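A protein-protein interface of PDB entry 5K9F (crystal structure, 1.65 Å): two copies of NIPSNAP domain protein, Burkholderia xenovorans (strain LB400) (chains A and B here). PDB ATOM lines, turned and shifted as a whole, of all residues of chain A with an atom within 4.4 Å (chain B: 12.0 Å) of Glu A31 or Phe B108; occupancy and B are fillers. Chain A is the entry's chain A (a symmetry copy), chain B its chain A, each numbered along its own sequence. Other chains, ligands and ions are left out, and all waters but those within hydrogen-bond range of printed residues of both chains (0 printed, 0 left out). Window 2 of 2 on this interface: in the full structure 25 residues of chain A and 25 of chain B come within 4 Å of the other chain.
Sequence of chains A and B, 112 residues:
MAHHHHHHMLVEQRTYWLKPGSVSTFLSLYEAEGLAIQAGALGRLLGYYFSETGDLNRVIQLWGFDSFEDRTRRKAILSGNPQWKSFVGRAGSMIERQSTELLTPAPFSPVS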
ATOM      1  N   LEU A  27     -20.716 -12.377  22.407  1.00  0.00           N
ATOM      2  CA  LEU A  27     -19.684 -12.044  23.386  1.00  0.00           C
ATOM      3  C   LEU A  27     -20.293 -11.668  24.731  1.00  0.00           C
ATOM      4  O   LEU A  27     -19.738 -12.004  25.777  1.00  0.00           O
ATOM      5  CB  LEU A  27     -18.798 -10.909  22.866  1.00  0.00           C
ATOM      6  CG  LEU A  27     -17.880 -11.315  21.708  1.00  0.00           C
ATOM      7  CD1 LEU A  27     -17.116 -10.091  21.210  1.00  0.00           C
ATOM      8  CD2 LEU A  27     -16.926 -12.437  22.127  1.00  0.00           C
ATOM      9  N   SER A  28     -21.424 -10.962  24.720  1.00  0.00           N
ATOM     10  CA  SER A  28     -22.088 -10.618  25.974  1.00  0.00           C
ATOM     11  C   SER A  28     -22.613 -11.858  26.683  1.00  0.00           C
ATOM     12  O   SER A  28     -22.469 -11.988  27.907  1.00  0.00           O
ATOM     13  CB  SER A  28     -23.227  -9.636  25.711  1.00  0.00           C
ATOM     14  OG  SER A  28     -22.717  -8.380  25.316  1.00  0.00           O
ATOM     15  N   LEU A  29     -23.238 -12.767  25.937  1.00  0.00           N
ATOM     16  CA  LEU A  29     -23.775 -13.988  26.530  1.00  0.00           C
ATOM     17  C   LEU A  29     -22.656 -14.880  27.049  1.00  0.00           C
ATOM     18  O   LEU A  29     -22.763 -15.447  28.147  1.00  0.00           O
ATOM     19  CB  LEU A  29     -24.623 -14.726  25.495  1.00  0.00           C
ATOM     20  CG  LEU A  29     -25.400 -15.964  25.933  1.00  0.00           C
ATOM     21  CD1 LEU A  29     -26.429 -15.633  26.999  1.00  0.00           C
ATOM     22  CD2 LEU A  29     -26.070 -16.571  24.709  1.00  0.00           C
ATOM     23  N   TYR A  30     -21.573 -15.008  26.278  1.00  0.00           N
ATOM     24  CA  TYR A  30     -20.425 -15.798  26.713  1.00  0.00           C
ATOM     25  C   TYR A  30     -19.808 -15.227  27.987  1.00  0.00           C
ATOM     26  O   TYR A  30     -19.539 -15.962  28.946  1.00  0.00           O
ATOM     27  CB  TYR A  30     -19.382 -15.870  25.584  1.00  0.00           C
ATOM     28  CG  TYR A  30     -18.102 -16.568  26.010  1.00  0.00           C
ATOM     29  CD1 TYR A  30     -18.057 -17.948  26.162  1.00  0.00           C
ATOM     30  CD2 TYR A  30     -16.949 -15.841  26.292  1.00  0.00           C
ATOM     31  CE1 TYR A  30     -16.892 -18.586  26.562  1.00  0.00           C
ATOM     32  CE2 TYR A  30     -15.782 -16.468  26.695  1.00  0.00           C
ATOM     33  CZ  TYR A  30     -15.757 -17.844  26.819  1.00  0.00           C
ATOM     34  OH  TYR A  30     -14.592 -18.472  27.217  1.00  0.00           O
ATOM     35  N   GLU A  31     -19.577 -13.911  28.026  1.00  0.00           N
ATOM     36  CA  GLU A  31     -18.948 -13.343  29.217  1.00  0.00           C
ATOM     37  C   GLU A  31     -19.811 -13.573  30.448  1.00  0.00           C
ATOM     38  O   GLU A  31     -19.297 -13.831  31.547  1.00  0.00           O
ATOM     39  CB  GLU A  31     -18.673 -11.849  29.032  1.00  0.00           C
ATOM     40  CG  GLU A  31     -17.897 -11.249  30.209  1.00  0.00           C
ATOM     41  CD  GLU A  31     -17.551  -9.775  30.038  1.00  0.00           C
ATOM     42  OE1 GLU A  31     -17.833  -9.194  28.970  1.00  0.00           O
ATOM     43  OE2 GLU A  31     -16.989  -9.193  30.993  1.00  0.00           O
ATOM     44  N   ALA A  32     -21.133 -13.508  30.283  1.00  0.00           N
ATOM     45  CA  ALA A  32     -22.018 -13.637  31.432  1.00  0.00           C
ATOM     46  C   ALA A  32     -22.204 -15.085  31.874  1.00  0.00           C
ATOM     47  O   ALA A  32     -22.380 -15.340  33.073  1.00  0.00           O
ATOM     48  CB  ALA A  32     -23.378 -13.016  31.112  1.00  0.00           C
ATOM     49  N   GLU A  33     -22.171 -16.041  30.940  1.00  0.00           N
ATOM     50  CA  GLU A  33     -22.602 -17.408  31.220  1.00  0.00           C
ATOM     51  C   GLU A  33     -21.586 -18.493  30.884  1.00  0.00           C
ATOM     52  O   GLU A  33     -21.756 -19.622  31.364  1.00  0.00           O
ATOM     53  CB  GLU A  33     -23.901 -17.723  30.462  1.00  0.00           C
ATOM     54  CG  GLU A  33     -25.033 -16.742  30.721  1.00  0.00           C
ATOM     55  CD  GLU A  33     -26.353 -17.200  30.125  1.00  0.00           C
ATOM     56  OE1 GLU A  33     -26.389 -18.303  29.541  1.00  0.00           O
ATOM     57  OE2 GLU A  33     -27.354 -16.459  30.242  1.00  0.00           O
ATOM     58  N   LEU A  35     -17.731 -17.828  30.153  1.00  0.00           N
ATOM     59  CA  LEU A  35     -16.307 -17.554  30.347  1.00  0.00           C
ATOM     60  C   LEU A  35     -15.760 -18.207  31.617  1.00  0.00           C
ATOM     61  O   LEU A  35     -14.724 -18.883  31.581  1.00  0.00           O
ATOM     62  CB  LEU A  35     -16.074 -16.042  30.388  1.00  0.00           C
ATOM     63  CG  LEU A  35     -14.674 -15.591  30.795  1.00  0.00           C
ATOM     64  CD1 LEU A  35     -13.617 -16.094  29.810  1.00  0.00           C
ATOM     65  CD2 LEU A  35     -14.634 -14.075  30.907  1.00  0.00           C
ATOM     66  N   TYR A  48      -8.884 -13.552  23.181  1.00  0.00           N
ATOM     67  CA  TYR A  48     -10.251 -13.778  22.718  1.00  0.00           C
ATOM     68  C   TYR A  48     -10.634 -12.528  21.939  1.00  0.00           C
ATOM     69  O   TYR A  48     -10.704 -11.439  22.518  1.00  0.00           O
ATOM     70  CB  TYR A  48     -11.197 -14.029  23.899  1.00  0.00           C
ATOM     71  CG  TYR A  48     -12.415 -14.885  23.598  1.00  0.00           C
ATOM     72  CD1 TYR A  48     -13.425 -14.428  22.772  1.00  0.00           C
ATOM     73  CD2 TYR A  48     -12.571 -16.134  24.187  1.00  0.00           C
ATOM     74  CE1 TYR A  48     -14.551 -15.206  22.524  1.00  0.00           C
ATOM     75  CE2 TYR A  48     -13.676 -16.917  23.936  1.00  0.00           C
ATOM     76  CZ  TYR A  48     -14.667 -16.456  23.104  1.00  0.00           C
ATOM     77  OH  TYR A  48     -15.779 -17.236  22.851  1.00  0.00           O
ATOM     78  N   MET B   9      -7.055  -1.702  22.454  1.00  0.00           N
ATOM     79  CA  MET B   9      -5.905  -2.212  21.720  1.00  0.00           C
ATOM     80  C   MET B   9      -6.334  -2.753  20.342  1.00  0.00           C
ATOM     81  O   MET B   9      -7.404  -3.331  20.178  1.00  0.00           O
ATOM     82  CB  MET B   9      -5.183  -3.303  22.531  1.00  0.00           C
ATOM     83  CG  MET B   9      -3.935  -3.880  21.846  1.00  0.00           C
ATOM     84  SD  MET B   9      -2.881  -4.974  22.848  1.00  0.00           S
ATOM     85  CE  MET B   9      -3.881  -6.462  22.994  1.00  0.00           C
ATOM     86  N   VAL B  11      -5.165  -5.414  17.491  1.00  0.00           N
ATOM     87  CA  VAL B  11      -4.310  -6.590  17.380  1.00  0.00           C
ATOM     88  C   VAL B  11      -4.163  -6.976  15.916  1.00  0.00           C
ATOM     89  O   VAL B  11      -5.154  -7.058  15.179  1.00  0.00           O
ATOM     90  CB  VAL B  11      -4.862  -7.754  18.221  1.00  0.00           C
ATOM     91  CG1 VAL B  11      -4.058  -8.996  17.983  1.00  0.00           C
ATOM     92  CG2 VAL B  11      -4.811  -7.387  19.705  1.00  0.00           C
ATOM     93  N   THR B 104      -9.980  -7.189  17.228  1.00  0.00           N
ATOM     94  CA  THR B 104     -10.252  -6.406  18.429  1.00  0.00           C
ATOM     95  C   THR B 104     -10.439  -7.344  19.610  1.00  0.00           C
ATOM     96  O   THR B 104     -11.193  -8.318  19.504  1.00  0.00           O
ATOM     97  CB  THR B 104     -11.507  -5.567  18.249  1.00  0.00           C
ATOM     98  OG1 THR B 104     -11.295  -4.630  17.192  1.00  0.00           O
ATOM     99  CG2 THR B 104     -11.827  -4.810  19.547  1.00  0.00           C
ATOM    100  N   PRO B 105      -9.767  -7.110  20.736  1.00  0.00           N
ATOM    101  CA  PRO B 105      -9.992  -7.967  21.905  1.00  0.00           C
ATOM    102  C   PRO B 105     -11.392  -7.778  22.469  1.00  0.00           C
ATOM    103  O   PRO B 105     -11.912  -6.658  22.535  1.00  0.00           O
ATOM    104  CB  PRO B 105      -8.925  -7.501  22.907  1.00  0.00           C
ATOM    105  CG  PRO B 105      -7.926  -6.726  22.095  1.00  0.00           C
ATOM    106  CD  PRO B 105      -8.694  -6.127  20.955  1.00  0.00           C
ATOM    107  N   ALA B 106     -11.998  -8.894  22.878  1.00  0.00           N
ATOM    108  CA  ALA B 106     -13.174  -8.837  23.725  1.00  0.00           C
ATOM    109  C   ALA B 106     -12.804  -8.165  25.048  1.00  0.00           C
ATOM    110  O   ALA B 106     -11.636  -8.154  25.445  1.00  0.00           O
ATOM    111  CB  ALA B 106     -13.718 -10.244  23.961  1.00  0.00           C
ATOM    112  N   PRO B 107     -13.787  -7.583  25.743  1.00  0.00           N
ATOM    113  CA  PRO B 107     -13.475  -6.860  26.989  1.00  0.00           C
ATOM    114  C   PRO B 107     -12.764  -7.700  28.040  1.00  0.00           C
ATOM    115  O   PRO B 107     -11.965  -7.165  28.821  1.00  0.00           O
ATOM    116  CB  PRO B 107     -14.858  -6.410  27.478  1.00  0.00           C
ATOM    117  CG  PRO B 107     -15.688  -6.323  26.234  1.00  0.00           C
ATOM    118  CD  PRO B 107     -15.184  -7.402  25.315  1.00  0.00           C
ATOM    119  N   PHE B 108     -13.037  -8.998  28.084  1.00  0.00           N
ATOM    120  CA  PHE B 108     -12.481  -9.919  29.067  1.00  0.00           C
ATOM    121  C   PHE B 108     -11.193 -10.592  28.594  1.00  0.00           C
ATOM    122  O   PHE B 108     -10.638 -11.418  29.329  1.00  0.00           O
ATOM    123  CB  PHE B 108     -13.523 -10.994  29.394  1.00  0.00           C
ATOM    124  CG  PHE B 108     -14.021 -11.720  28.175  1.00  0.00           C
ATOM    125  CD1 PHE B 108     -13.301 -12.782  27.645  1.00  0.00           C
ATOM    126  CD2 PHE B 108     -15.183 -11.316  27.534  1.00  0.00           C
ATOM    127  CE1 PHE B 108     -13.738 -13.434  26.503  1.00  0.00           C
ATOM    128  CE2 PHE B 108     -15.630 -11.972  26.394  1.00  0.00           C
ATOM    129  CZ  PHE B 108     -14.899 -13.030  25.875  1.00  0.00           C
ATOM    130  N   SER B 109     -10.730 -10.292  27.385  1.00  0.00           N
ATOM    131  CA  SER B 109      -9.488 -10.877  26.896  1.00  0.00           C
ATOM    132  C   SER B 109      -8.321 -10.407  27.764  1.00  0.00           C
ATOM    133  O   SER B 109      -8.316  -9.258  28.227  1.00  0.00           O
ATOM    134  CB  SER B 109      -9.272 -10.489  25.426  1.00  0.00           C
ATOM    135  OG  SER B 109      -8.154 -11.148  24.835  1.00  0.00           O
ATOM    136  N   PRO B 110      -7.322 -11.256  28.015  1.00  0.00           N
ATOM    137  CA  PRO B 110      -6.318 -10.936  29.038  1.00  0.00           C
ATOM    138  C   PRO B 110      -5.388  -9.802  28.627  1.00  0.00           C
ATOM    139  O   PRO B 110      -5.283  -9.431  27.456  1.00  0.00           O
ATOM    140  CB  PRO B 110      -5.545 -12.248  29.209  1.00  0.00           C
ATOM    141  CG  PRO B 110      -5.722 -12.962  27.911  1.00  0.00           C
ATOM    142  CD  PRO B 110      -7.106 -12.591  27.426  1.00  0.00           C
ATOM    143  N   VAL B 111      -4.704  -9.257  29.634  1.00  0.00           N
ATOM    144  CA  VAL B 111      -3.729  -8.178  29.467  1.00  0.00           C
ATOM    145  C   VAL B 111      -4.380  -6.936  28.871  1.00  0.00           C
ATOM    146  O   VAL B 111      -4.388  -5.870  29.491  1.00  0.00           O
ATOM    147  CB  VAL B 111      -2.530  -8.630  28.604  1.00  0.00           C
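The backbone NH (N) of Ala B106 lies within hydrogen-bond range of the backbone carbonyl oxygen (O) of Tyr A48.
OG of Ser B109 sits at hydrogen-bond distance from N of Tyr A48 (3.0 Å).
Of the printed residues of chain B, Glu A31 touches Phe B108 (3.7 Å).
Of chain A, only Tyr A30 (3.5 Å), Glu A31 (3.7 Å), Leu A35 (3.6 Å) and Tyr A48 (3.5 Å) come within 4 Å of Phe B108.
No residue of chain B comes within 4 Å of Leu A27.
Tyr A30 touches just one residue of chain B: Phe B108.
Leu A35 touches one residue of chain B.
Of the printed residues of chain B, Tyr A48 touches Pro B105 (3.6 Å), Ala B106 (2.9 Å), Phe B108 (3.5 Å) and Ser B109 (3.0 Å).
Of the printed residues of chain A, Ser B109 touches Tyr A48 (3.0 Å).
Printed residues of chain A within 4 Å of Pro B105: Tyr A48 (3.6 Å).
Printed residues of chain A within 4 Å of Ala B106: Tyr A48 (2.9 Å).
Met B9 touches none of the printed residues of chain A.
The nearest residue of chain A that does not touch Phe B108 is Leu A27 (4.2 Å).
N of Leu A35 is in hydrogen-bond range of O of Tyr A30, 2.9 Å away.
No position is printed for both chains.
Of the 7 pairs that touch across the chains among the printed residues, none has its exchanged pair printed and touching as well.
Of the 9 printed residues of chain A, 4 touch a printed residue of chain B.
Tyr A30 touches Phe B108.
Glu A31 touches Phe B108 (OE1 to CD2, 3.7 Å).
Leu A35 touches Phe B108 (CD2 to CB, 3.6 Å).
Pro B105 touches Tyr A48 (CA to O, 3.6 Å).
CE1 of Phe B108 touches CG of Tyr A48, at 3.5 Å.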
